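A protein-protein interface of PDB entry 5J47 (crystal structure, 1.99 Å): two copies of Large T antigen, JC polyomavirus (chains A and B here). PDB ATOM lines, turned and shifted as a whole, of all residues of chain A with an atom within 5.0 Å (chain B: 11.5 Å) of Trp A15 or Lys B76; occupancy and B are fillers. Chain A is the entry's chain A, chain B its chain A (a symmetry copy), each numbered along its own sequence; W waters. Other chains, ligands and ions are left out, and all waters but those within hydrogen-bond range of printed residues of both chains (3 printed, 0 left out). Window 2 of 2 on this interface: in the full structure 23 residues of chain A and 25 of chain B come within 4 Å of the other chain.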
ATOM      1  N   GLN A  12      -5.488  -2.271  16.417  1.00  0.00           N
ATOM      2  CA  GLN A  12      -5.931  -1.979  17.774  1.00  0.00           C
ATOM      3  C   GLN A  12      -7.459  -1.869  17.830  1.00  0.00           C
ATOM      4  O   GLN A  12      -8.064  -1.205  16.986  1.00  0.00           O
ATOM      5  CB  GLN A  12      -5.260  -0.687  18.284  1.00  0.00           C
ATOM      6  CG  GLN A  12      -5.499  -0.371  19.766  1.00  0.00           C
ATOM      7  CD  GLN A  12      -4.987  -1.455  20.681  1.00  0.00           C
ATOM      8  OE1 GLN A  12      -3.776  -1.651  20.840  1.00  0.00           O
ATOM      9  NE2 GLN A  12      -5.904  -2.198  21.283  1.00  0.00           N
ATOM     10  N   VAL A  13      -8.069  -2.527  18.825  1.00  0.00           N
ATOM     11  CA  VAL A  13      -9.517  -2.508  19.038  1.00  0.00           C
ATOM     12  C   VAL A  13      -9.938  -1.211  19.744  1.00  0.00           C
ATOM     13  O   VAL A  13      -9.290  -0.782  20.705  1.00  0.00           O
ATOM     14  CB  VAL A  13     -10.030  -3.802  19.745  1.00  0.00           C
ATOM     15  CG1 VAL A  13      -9.253  -4.100  21.022  1.00  0.00           C
ATOM     16  CG2 VAL A  13     -11.532  -3.754  20.016  1.00  0.00           C
ATOM     17  N   SER A  14     -11.018  -0.579  19.257  1.00  0.00           N
ATOM     18  CA  SER A  14     -11.494   0.639  19.891  1.00  0.00           C
ATOM     19  C   SER A  14     -12.373   0.272  21.092  1.00  0.00           C
ATOM     20  O   SER A  14     -13.507  -0.185  20.911  1.00  0.00           O
ATOM     21  CB  SER A  14     -12.242   1.523  18.897  1.00  0.00           C
ATOM     22  OG  SER A  14     -12.813   2.626  19.577  1.00  0.00           O
ATOM     23  N   TRP A  15     -11.825   0.444  22.317  1.00  0.00           N
ATOM     24  CA  TRP A  15     -12.552   0.171  23.559  1.00  0.00           C
ATOM     25  C   TRP A  15     -13.735   1.144  23.659  1.00  0.00           C
ATOM     26  O   TRP A  15     -14.810   0.748  24.107  1.00  0.00           O
ATOM     27  CB  TRP A  15     -11.633   0.330  24.780  1.00  0.00           C
ATOM     28  CG  TRP A  15     -10.621  -0.766  24.980  1.00  0.00           C
ATOM     29  CD1 TRP A  15      -9.767  -1.281  24.048  1.00  0.00           C
ATOM     30  CD2 TRP A  15     -10.267  -1.377  26.229  1.00  0.00           C
ATOM     31  NE1 TRP A  15      -8.943  -2.218  24.627  1.00  0.00           N
ATOM     32  CE2 TRP A  15      -9.207  -2.276  25.970  1.00  0.00           C
ATOM     33  CE3 TRP A  15     -10.741  -1.251  27.546  1.00  0.00           C
ATOM     34  CZ2 TRP A  15      -8.636  -3.070  26.977  1.00  0.00           C
ATOM     35  CZ3 TRP A  15     -10.187  -2.052  28.536  1.00  0.00           C
ATOM     36  CH2 TRP A  15      -9.155  -2.954  28.248  1.00  0.00           C
ATOM     37  N   LYS A  16     -13.525   2.411  23.222  1.00  0.00           N
ATOM     38  CA  LYS A  16     -14.524   3.482  23.195  1.00  0.00           C
ATOM     39  C   LYS A  16     -15.758   3.074  22.376  1.00  0.00           C
ATOM     40  O   LYS A  16     -16.874   3.288  22.835  1.00  0.00           O
ATOM     41  CB  LYS A  16     -13.896   4.779  22.656  1.00  0.00           C
ATOM     42  CG  LYS A  16     -14.762   6.024  22.823  1.00  0.00           C
ATOM     43  CD  LYS A  16     -13.976   7.325  22.624  1.00  0.00           C
ATOM     44  CE  LYS A  16     -13.902   7.788  21.187  1.00  0.00           C
ATOM     45  NZ  LYS A  16     -12.799   7.127  20.444  1.00  0.00           N
ATOM     46  N   LEU A  17     -15.555   2.460  21.190  1.00  0.00           N
ATOM     47  CA  LEU A  17     -16.631   1.989  20.307  1.00  0.00           C
ATOM     48  C   LEU A  17     -17.436   0.832  20.922  1.00  0.00           C
ATOM     49  O   LEU A  17     -18.652   0.773  20.739  1.00  0.00           O
ATOM     50  CB  LEU A  17     -16.065   1.549  18.946  1.00  0.00           C
ATOM     51  CG  LEU A  17     -16.506   2.276  17.666  1.00  0.00           C
ATOM     52  CD1 LEU A  17     -16.418   1.344  16.476  1.00  0.00           C
ATOM     53  CD2 LEU A  17     -17.935   2.839  17.756  1.00  0.00           C
ATOM     54  N   VAL A  18     -16.764  -0.095  21.628  1.00  0.00           N
ATOM     55  CA  VAL A  18     -17.431  -1.216  22.303  1.00  0.00           C
ATOM     56  C   VAL A  18     -18.302  -0.625  23.427  1.00  0.00           C
ATOM     57  O   VAL A  18     -19.450  -1.033  23.593  1.00  0.00           O
ATOM     58  CB  VAL A  18     -16.441  -2.299  22.824  1.00  0.00           C
ATOM     59  CG1 VAL A  18     -17.181  -3.452  23.494  1.00  0.00           C
ATOM     60  CG2 VAL A  18     -15.558  -2.828  21.696  1.00  0.00           C
ATOM     61  N   THR A  19     -17.749   0.365  24.165  1.00  0.00           N
ATOM     62  CA  THR A  19     -18.435   1.111  25.221  1.00  0.00           C
ATOM     63  C   THR A  19     -19.654   1.840  24.628  1.00  0.00           C
ATOM     64  O   THR A  19     -20.730   1.806  25.225  1.00  0.00           O
ATOM     65  CB  THR A  19     -17.448   2.070  25.892  1.00  0.00           C
ATOM     66  OG1 THR A  19     -16.480   1.321  26.636  1.00  0.00           O
ATOM     67  CG2 THR A  19     -18.129   3.083  26.781  1.00  0.00           C
ATOM     68  N   ASN A  77      -7.867  -9.971  25.069  1.00  0.00           N
ATOM     69  CA  ASN A  77      -8.350  -9.274  26.260  1.00  0.00           C
ATOM     70  C   ASN A  77      -9.826  -8.898  26.137  1.00  0.00           C
ATOM     71  O   ASN A  77     -10.221  -7.811  26.560  1.00  0.00           O
ATOM     72  CB  ASN A  77      -7.466  -8.026  26.510  1.00  0.00           C
ATOM     73  CG  ASN A  77      -7.369  -7.584  27.953  1.00  0.00           C
ATOM     74  OD1 ASN A  77      -7.113  -6.410  28.249  1.00  0.00           O
ATOM     75  ND2 ASN A  77      -7.584  -8.502  28.890  1.00  0.00           N
ATOM     76  N   SER A  80     -11.953  -7.991  29.495  1.00  0.00           N
ATOM     77  CA  SER A  80     -11.553  -6.689  30.042  1.00  0.00           C
ATOM     78  C   SER A  80     -12.136  -5.514  29.262  1.00  0.00           C
ATOM     79  O   SER A  80     -12.536  -4.525  29.876  1.00  0.00           O
ATOM     80  CB  SER A  80     -10.040  -6.572  30.131  1.00  0.00           C
ATOM     81  OG  SER A  80      -9.545  -7.525  31.053  1.00  0.00           O
ATOM     82  N   ILE A  81     -12.171  -5.611  27.919  1.00  0.00           N
ATOM     83  CA  ILE A  81     -12.753  -4.583  27.045  1.00  0.00           C
ATOM     84  C   ILE A  81     -14.236  -4.413  27.415  1.00  0.00           C
ATOM     85  O   ILE A  81     -14.710  -3.284  27.583  1.00  0.00           O
ATOM     86  CB  ILE A  81     -12.579  -4.952  25.540  1.00  0.00           C
ATOM     87  CG1 ILE A  81     -11.086  -5.015  25.143  1.00  0.00           C
ATOM     88  CG2 ILE A  81     -13.352  -3.972  24.635  1.00  0.00           C
ATOM     89  CD1 ILE A  81     -10.811  -5.824  23.891  1.00  0.00           C
ATOM     90  N   GLN A  84     -14.914  -2.803  31.032  1.00  0.00           N
ATOM     91  CA  GLN A  84     -14.850  -1.341  31.023  1.00  0.00           C
ATOM     92  C   GLN A  84     -16.118  -0.752  30.394  1.00  0.00           C
ATOM     93  O   GLN A  84     -16.622   0.263  30.876  1.00  0.00           O
ATOM     94  CB  GLN A  84     -13.587  -0.821  30.325  1.00  0.00           C
ATOM     95  CG  GLN A  84     -13.533   0.715  30.294  1.00  0.00           C
ATOM     96  CD  GLN A  84     -12.196   1.245  29.893  1.00  0.00           C
ATOM     97  OE1 GLN A  84     -11.230   1.161  30.646  1.00  0.00           O
ATOM     98  NE2 GLN A  84     -12.129   1.870  28.725  1.00  0.00           N
ATOM     99  N   THR B  10       1.466   7.963  21.404  1.00  0.00           N
ATOM    100  CA  THR B  10       0.077   8.221  21.783  1.00  0.00           C
ATOM    101  C   THR B  10      -0.025   9.190  22.969  1.00  0.00           C
ATOM    102  O   THR B  10       0.896   9.263  23.792  1.00  0.00           O
ATOM    103  CB  THR B  10      -0.652   6.903  22.066  1.00  0.00           C
ATOM    104  N   LYS B  11      -1.152   9.935  23.050  1.00  0.00           N
ATOM    105  CA  LYS B  11      -1.417  10.898  24.124  1.00  0.00           C
ATOM    106  C   LYS B  11      -1.578  10.199  25.471  1.00  0.00           C
ATOM    107  O   LYS B  11      -2.159   9.114  25.545  1.00  0.00           O
ATOM    108  CB  LYS B  11      -2.637  11.781  23.809  1.00  0.00           C
ATOM    109  CG  LYS B  11      -2.329  12.913  22.839  1.00  0.00           C
ATOM    110  CD  LYS B  11      -3.505  13.865  22.676  1.00  0.00           C
ATOM    111  CE  LYS B  11      -3.206  14.959  21.680  1.00  0.00           C
ATOM    112  NZ  LYS B  11      -4.279  15.987  21.644  1.00  0.00           N
ATOM    113  N   GLN B  12      -1.021  10.805  26.522  1.00  0.00           N
ATOM    114  CA  GLN B  12      -1.061  10.280  27.880  1.00  0.00           C
ATOM    115  C   GLN B  12      -2.061  11.068  28.734  1.00  0.00           C
ATOM    116  O   GLN B  12      -2.064  12.300  28.706  1.00  0.00           O
ATOM    117  CB  GLN B  12       0.351  10.315  28.503  1.00  0.00           C
ATOM    118  CG  GLN B  12       0.480   9.618  29.862  1.00  0.00           C
ATOM    119  CD  GLN B  12       0.125   8.153  29.800  1.00  0.00           C
ATOM    120  OE1 GLN B  12       0.851   7.333  29.227  1.00  0.00           O
ATOM    121  NE2 GLN B  12      -1.017   7.800  30.372  1.00  0.00           N
ATOM    122  N   VAL B  13      -2.906  10.345  29.482  1.00  0.00           N
ATOM    123  CA  VAL B  13      -3.907  10.937  30.371  1.00  0.00           C
ATOM    124  C   VAL B  13      -3.254  11.390  31.685  1.00  0.00           C
ATOM    125  O   VAL B  13      -2.445  10.659  32.267  1.00  0.00           O
ATOM    126  CB  VAL B  13      -5.146  10.009  30.572  1.00  0.00           C
ATOM    127  CG1 VAL B  13      -4.741   8.603  30.999  1.00  0.00           C
ATOM    128  CG2 VAL B  13      -6.161  10.606  31.544  1.00  0.00           C
ATOM    129  N   SER B  14      -3.598  12.604  32.147  1.00  0.00           N
ATOM    130  CA  SER B  14      -3.044  13.089  33.400  1.00  0.00           C
ATOM    131  C   SER B  14      -3.864  12.524  34.565  1.00  0.00           C
ATOM    132  O   SER B  14      -4.997  12.960  34.792  1.00  0.00           O
ATOM    133  CB  SER B  14      -3.002  14.613  33.430  1.00  0.00           C
ATOM    134  OG  SER B  14      -2.593  15.052  34.715  1.00  0.00           O
ATOM    135  N   TRP B  15      -3.293  11.524  35.277  1.00  0.00           N
ATOM    136  CA  TRP B  15      -3.936  10.908  36.440  1.00  0.00           C
ATOM    137  C   TRP B  15      -4.082  11.968  37.540  1.00  0.00           C
ATOM    138  O   TRP B  15      -5.100  11.989  38.231  1.00  0.00           O
ATOM    139  CB  TRP B  15      -3.112   9.719  36.958  1.00  0.00           C
ATOM    140  CG  TRP B  15      -3.158   8.476  36.111  1.00  0.00           C
ATOM    141  CD1 TRP B  15      -2.964   8.389  34.762  1.00  0.00           C
ATOM    142  CD2 TRP B  15      -3.274   7.128  36.587  1.00  0.00           C
ATOM    143  NE1 TRP B  15      -3.012   7.074  34.361  1.00  0.00           N
ATOM    144  CE2 TRP B  15      -3.172   6.276  35.464  1.00  0.00           C
ATOM    145  CE3 TRP B  15      -3.455   6.554  37.857  1.00  0.00           C
ATOM    146  CZ2 TRP B  15      -3.276   4.880  35.570  1.00  0.00           C
ATOM    147  CZ3 TRP B  15      -3.577   5.174  37.957  1.00  0.00           C
ATOM    148  CH2 TRP B  15      -3.497   4.354  36.824  1.00  0.00           C
ATOM    149  N   MET B  34     -15.965   8.406  37.216  1.00  0.00           N
ATOM    150  CA  MET B  34     -15.828   7.930  35.842  1.00  0.00           C
ATOM    151  C   MET B  34     -16.883   8.556  34.923  1.00  0.00           C
ATOM    152  O   MET B  34     -16.540   9.091  33.865  1.00  0.00           O
ATOM    153  CB  MET B  34     -15.936   6.401  35.840  1.00  0.00           C
ATOM    154  CG  MET B  34     -15.386   5.767  34.616  1.00  0.00           C
ATOM    155  SD  MET B  34     -15.260   3.975  34.867  1.00  0.00           S
ATOM    156  CE  MET B  34     -15.532   3.455  33.231  1.00  0.00           C
ATOM    157  N   LEU B  38     -16.140  11.452  32.056  1.00  0.00           N
ATOM    158  CA  LEU B  38     -16.480  11.177  30.664  1.00  0.00           C
ATOM    159  C   LEU B  38     -17.373  12.284  30.076  1.00  0.00           C
ATOM    160  O   LEU B  38     -17.249  12.595  28.895  1.00  0.00           O
ATOM    161  CB  LEU B  38     -17.118   9.791  30.484  1.00  0.00           C
ATOM    162  CG  LEU B  38     -16.149   8.610  30.508  1.00  0.00           C
ATOM    163  CD1 LEU B  38     -16.902   7.312  30.668  1.00  0.00           C
ATOM    164  CD2 LEU B  38     -15.277   8.560  29.243  1.00  0.00           C
ATOM    165  N   GLN B  41     -15.706  15.258  27.900  1.00  0.00           N
ATOM    166  CA  GLN B  41     -15.080  15.005  26.591  1.00  0.00           C
ATOM    167  C   GLN B  41     -15.636  15.848  25.414  1.00  0.00           C
ATOM    168  O   GLN B  41     -14.913  16.039  24.438  1.00  0.00           O
ATOM    169  CB  GLN B  41     -15.095  13.508  26.237  1.00  0.00           C
ATOM    170  CG  GLN B  41     -16.424  12.967  25.710  1.00  0.00           C
ATOM    171  CD  GLN B  41     -16.337  11.494  25.399  1.00  0.00           C
ATOM    172  OE1 GLN B  41     -16.800  10.646  26.169  1.00  0.00           O
ATOM    173  NE2 GLN B  41     -15.734  11.158  24.266  1.00  0.00           N
ATOM    174  N   ASN B  68      -8.090  16.674  28.778  1.00  0.00           N
ATOM    175  CA  ASN B  68      -7.757  15.462  29.528  1.00  0.00           C
ATOM    176  C   ASN B  68      -8.875  14.414  29.437  1.00  0.00           C
ATOM    177  O   ASN B  68      -8.586  13.217  29.431  1.00  0.00           O
ATOM    178  CB  ASN B  68      -7.462  15.793  30.984  1.00  0.00           C
ATOM    179  CG  ASN B  68      -6.618  14.755  31.673  1.00  0.00           C
ATOM    180  OD1 ASN B  68      -5.639  14.250  31.122  1.00  0.00           O
ATOM    181  ND2 ASN B  68      -6.962  14.430  32.908  1.00  0.00           N
ATOM    182  N   ALA B  69     -10.145  14.865  29.379  1.00  0.00           N
ATOM    183  CA  ALA B  69     -11.319  13.994  29.276  1.00  0.00           C
ATOM    184  C   ALA B  69     -11.395  13.327  27.913  1.00  0.00           C
ATOM    185  O   ALA B  69     -11.861  12.194  27.823  1.00  0.00           O
ATOM    186  CB  ALA B  69     -12.583  14.779  29.547  1.00  0.00           C
ATOM    187  N   GLN B  70     -10.925  14.019  26.853  1.00  0.00           N
ATOM    188  CA  GLN B  70     -10.869  13.467  25.498  1.00  0.00           C
ATOM    189  C   GLN B  70      -9.878  12.297  25.489  1.00  0.00           C
ATOM    190  O   GLN B  70     -10.190  11.240  24.941  1.00  0.00           O
ATOM    191  CB  GLN B  70     -10.452  14.536  24.481  1.00  0.00           C
ATOM    192  CG  GLN B  70     -11.568  15.514  24.115  1.00  0.00           C
ATOM    193  CD  GLN B  70     -11.127  16.505  23.067  1.00  0.00           C
ATOM    194  OE1 GLN B  70     -10.202  17.301  23.265  1.00  0.00           O
ATOM    195  NE2 GLN B  70     -11.795  16.493  21.928  1.00  0.00           N
ATOM    196  N   ILE B  71      -8.706  12.477  26.148  1.00  0.00           N
ATOM    197  CA  ILE B  71      -7.679  11.438  26.281  1.00  0.00           C
ATOM    198  C   ILE B  71      -8.221  10.305  27.164  1.00  0.00           C
ATOM    199  O   ILE B  71      -8.095   9.144  26.786  1.00  0.00           O
ATOM    200  CB  ILE B  71      -6.306  11.989  26.772  1.00  0.00           C
ATOM    201  CG1 ILE B  71      -5.843  13.195  25.916  1.00  0.00           C
ATOM    202  CG2 ILE B  71      -5.241  10.873  26.763  1.00  0.00           C
ATOM    203  CD1 ILE B  71      -4.764  14.098  26.575  1.00  0.00           C
ATOM    204  N   PHE B  72      -8.879  10.653  28.297  1.00  0.00           N
ATOM    205  CA  PHE B  72      -9.511   9.701  29.226  1.00  0.00           C
ATOM    206  C   PHE B  72     -10.511   8.795  28.490  1.00  0.00           C
ATOM    207  O   PHE B  72     -10.527   7.591  28.735  1.00  0.00           O
ATOM    208  CB  PHE B  72     -10.183  10.434  30.413  1.00  0.00           C
ATOM    209  CG  PHE B  72     -10.825   9.525  31.444  1.00  0.00           C
ATOM    210  CD1 PHE B  72     -10.055   8.899  32.421  1.00  0.00           C
ATOM    211  CD2 PHE B  72     -12.199   9.294  31.434  1.00  0.00           C
ATOM    212  CE1 PHE B  72     -10.645   8.041  33.357  1.00  0.00           C
ATOM    213  CE2 PHE B  72     -12.789   8.438  32.372  1.00  0.00           C
ATOM    214  CZ  PHE B  72     -12.010   7.828  33.335  1.00  0.00           C
ATOM    215  N   ALA B  73     -11.317   9.375  27.577  1.00  0.00           N
ATOM    216  CA  ALA B  73     -12.301   8.660  26.751  1.00  0.00           C
ATOM    217  C   ALA B  73     -11.673   7.535  25.904  1.00  0.00           C
ATOM    218  O   ALA B  73     -12.343   6.533  25.642  1.00  0.00           O
ATOM    219  CB  ALA B  73     -13.032   9.635  25.854  1.00  0.00           C
ATOM    220  N   ASP B  74     -10.406   7.715  25.470  1.00  0.00           N
ATOM    221  CA  ASP B  74      -9.637   6.749  24.676  1.00  0.00           C
ATOM    222  C   ASP B  74      -8.828   5.764  25.548  1.00  0.00           C
ATOM    223  O   ASP B  74      -8.177   4.874  24.998  1.00  0.00           O
ATOM    224  CB  ASP B  74      -8.676   7.487  23.708  1.00  0.00           C
ATOM    225  CG  ASP B  74      -9.344   8.280  22.594  1.00  0.00           C
ATOM    226  OD1 ASP B  74     -10.344   7.782  22.026  1.00  0.00           O
ATOM    227  OD2 ASP B  74      -8.827   9.367  22.246  1.00  0.00           O
ATOM    228  N   SER B  75      -8.857   5.926  26.888  1.00  0.00           N
ATOM    229  CA  SER B  75      -8.099   5.082  27.820  1.00  0.00           C
ATOM    230  C   SER B  75      -8.634   3.658  27.935  1.00  0.00           C
ATOM    231  O   SER B  75      -9.842   3.433  27.864  1.00  0.00           O
ATOM    232  CB  SER B  75      -8.021   5.730  29.201  1.00  0.00           C
ATOM    233  OG  SER B  75      -7.242   4.964  30.106  1.00  0.00           O
ATOM    234  N   LYS B  76      -7.717   2.706  28.153  1.00  0.00           N
ATOM    235  CA  LYS B  76      -8.010   1.283  28.331  1.00  0.00           C
ATOM    236  C   LYS B  76      -7.857   0.935  29.824  1.00  0.00           C
ATOM    237  O   LYS B  76      -7.901  -0.238  30.196  1.00  0.00           O
ATOM    238  CB  LYS B  76      -7.029   0.449  27.501  1.00  0.00           C
ATOM    239  CG  LYS B  76      -7.100   0.691  25.995  1.00  0.00           C
ATOM    240  CD  LYS B  76      -5.948  -0.017  25.280  1.00  0.00           C
ATOM    241  CE  LYS B  76      -6.001   0.161  23.782  1.00  0.00           C
ATOM    242  NZ  LYS B  76      -5.653   1.543  23.353  1.00  0.00           N
ATOM    243  N   ASN B  77      -7.692   1.972  30.681  1.00  0.00           N
ATOM    244  CA  ASN B  77      -7.482   1.803  32.118  1.00  0.00           C
ATOM    245  C   ASN B  77      -8.268   2.830  32.932  1.00  0.00           C
ATOM    246  O   ASN B  77      -7.760   3.343  33.930  1.00  0.00           O
ATOM    247  CB  ASN B  77      -5.964   1.880  32.421  1.00  0.00           C
ATOM    248  CG  ASN B  77      -5.511   1.110  33.642  1.00  0.00           C
ATOM    249  OD1 ASN B  77      -4.487   1.430  34.259  1.00  0.00           O
ATOM    250  ND2 ASN B  77      -6.263   0.086  34.033  1.00  0.00           N
ATOM    251  N   GLN B  78      -9.519   3.124  32.509  1.00  0.00           N
ATOM    252  CA  GLN B  78     -10.374   4.139  33.129  1.00  0.00           C
ATOM    253  C   GLN B  78     -10.682   3.913  34.608  1.00  0.00           C
ATOM    254  O   GLN B  78     -10.578   4.867  35.382  1.00  0.00           O
ATOM    255  CB  GLN B  78     -11.677   4.325  32.337  1.00  0.00           C
ATOM    256  CG  GLN B  78     -11.481   5.056  31.017  1.00  0.00           C
ATOM    257  CD  GLN B  78     -12.745   5.108  30.204  1.00  0.00           C
ATOM    258  OE1 GLN B  78     -13.778   4.535  30.560  1.00  0.00           O
ATOM    259  NE2 GLN B  78     -12.687   5.770  29.074  1.00  0.00           N
ATOM    260  N   LYS B  79     -11.075   2.677  35.003  1.00  0.00           N
ATOM    261  CA  LYS B  79     -11.386   2.350  36.404  1.00  0.00           C
ATOM    262  C   LYS B  79     -10.180   2.547  37.338  1.00  0.00           C
ATOM    263  O   LYS B  79     -10.357   3.074  38.441  1.00  0.00           O
ATOM    264  CB  LYS B  79     -11.980   0.936  36.557  1.00  0.00           C
ATOM    265  CG  LYS B  79     -12.772   0.768  37.855  1.00  0.00           C
ATOM    266  CD  LYS B  79     -13.220  -0.653  38.107  1.00  0.00           C
ATOM    267  CE  LYS B  79     -14.092  -0.715  39.336  1.00  0.00           C
ATOM    268  NZ  LYS B  79     -14.323  -2.113  39.785  1.00  0.00           N
ATOM    269  N   SER B  80      -8.964   2.148  36.891  1.00  0.00           N
ATOM    270  CA  SER B  80      -7.736   2.299  37.679  1.00  0.00           C
ATOM    271  C   SER B  80      -7.359   3.758  37.918  1.00  0.00           C
ATOM    272  O   SER B  80      -6.914   4.092  39.016  1.00  0.00           O
ATOM    273  CB  SER B  80      -6.577   1.546  37.044  1.00  0.00           C
ATOM    274  OG  SER B  80      -6.852   0.158  37.054  1.00  0.00           O
ATOM    275  N   ILE B  81      -7.520   4.620  36.896  1.00  0.00           N
ATOM    276  CA  ILE B  81      -7.252   6.061  36.999  1.00  0.00           C
ATOM    277  C   ILE B  81      -8.163   6.649  38.089  1.00  0.00           C
ATOM    278  O   ILE B  81      -7.694   7.395  38.955  1.00  0.00           O
ATOM    279  CB  ILE B  81      -7.466   6.777  35.629  1.00  0.00           C
ATOM    280  CG1 ILE B  81      -6.474   6.261  34.562  1.00  0.00           C
ATOM    281  CG2 ILE B  81      -7.368   8.309  35.782  1.00  0.00           C
ATOM    282  CD1 ILE B  81      -6.912   6.515  33.133  1.00  0.00           C
ATOM    283  N   CYS B  82      -9.462   6.288  38.039  1.00  0.00           N
ATOM    284  CA  CYS B  82     -10.485   6.727  38.985  1.00  0.00           C
ATOM    285  C   CYS B  82     -10.295   6.155  40.383  1.00  0.00           C
ATOM    286  O   CYS B  82     -10.615   6.850  41.343  1.00  0.00           O
ATOM    287  CB  CYS B  82     -11.878   6.445  38.444  1.00  0.00           C
ATOM    288  SG  CYS B  82     -12.281   7.409  36.974  1.00  0.00           S
HETATM  289  O   HOH W   1     -11.920   3.654  26.090  1.00  0.00           O
HETATM  290  O   HOH W   2     -10.365   3.167  23.094  1.00  0.00           O
HETATM  291  O   HOH W   3     -11.278   0.321  33.234  1.00  0.00           O
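OE1 of Gln A84 sits at hydrogen-bond distance from N of Gln B78. The side-chain carboxylate (OD1) of Asp B74 is in salt-bridge range of the side-chain amino group (NZ) of Lys A16 (3.0 Å). NE2 of Gln A84 sits at hydrogen-bond distance from O of Ser B75.
The backbone carbonyl oxygen of Trp A15 lies within hydrogen-bond range of the side-chain hydroxyl of Thr A19 (3.1 Å). ND2 of Asn B77 is in hydrogen-bond range of OG of Ser B80 (3.1 Å). SG of Cys B82 sits at hydrogen-bond distance from O of Gln B78, at 3.4 Å. N of Asn B77 lies within hydrogen-bond range of OG of Ser B75 (3.1 Å). The backbone carbonyl oxygen (O) of Phe B72 lies within hydrogen-bond range of the side-chain amide nitrogen (NE2) of Gln B78 (2.8 Å).
Among the printed residues, merely in contact across the chains: Gln A12 with Lys B76, Trp A15 with Lys B76, Lys A16 with Ala B73, Gln A84 with Lys B76 and Gln A84 with Asn B77.
Printed residues of chain B within 4 Å of Gln A12: Lys B76. No residue of chain B comes within 4 Å of Val A13. No residue of chain B comes within 4 Å of Ser A14. Trp A15 touches just one residue of chain B: Lys B76 (3.4 Å). Lys A16 touches two residues of chain B. No residue of chain B comes within 4 Å of Val A18. No residue of chain B comes within 4 Å of Ser A80. No residue of chain B comes within 4 Å of Ile A81. Asn B68 touches none of the printed residues of chain A. Lys B76 touches three residues of chain A. Of the printed residues of chain A, Gln B78 touches Gln A84 (3.2 Å). The nearest residue of chain A that does not touch Lys B76 is Val A13 (4.6 Å). The nearest printed residue of chain A that does not touch Ala B73 is Gln A84 (5.6 Å).
Of the 24 printed residues of chain B, 6 touch a printed residue of chain A. Along chain B the printed residues that touch a printed residue of chain A span positions 73 to 78. Printed residues of chain A that touch a printed residue of chain B: Gln A12, Trp A15, Lys A16 and Gln A84. Hydrophobic or aromatic side chains of chain A within 4 Å of the printed part of chain B: Trp A15. Along chain A the printed residues that touch a printed residue of chain B span positions 12 to 84. Among the printed residues, Asp or Glu carboxylates within 4 Å of a Lys or Arg side-chain nitrogen of the other chain: Lys A16 with Asp B74 (3.0 Å).
7 positions are printed for both chains.
Water W3 lies within hydrogen-bond range of the side-chain amide oxygen of Gln A84, the backbone NH of Lys B79 and the backbone NH of Gln B78. Water W1 lies within hydrogen-bond range of the backbone carbonyl oxygen of Ser B75 (2.7 Å), the backbone carbonyl oxygen of Ala B73 (2.9 Å) and the side-chain amide nitrogen of Gln A84 (3.2 Å). Water W2 lies within hydrogen-bond range of the backbone NH (N) of Trp A15 (3.2 Å), the backbone NH (N) of Lys A16 (3.3 Å) and the backbone carbonyl oxygen (O) of Asp B74 (3.4 Å).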
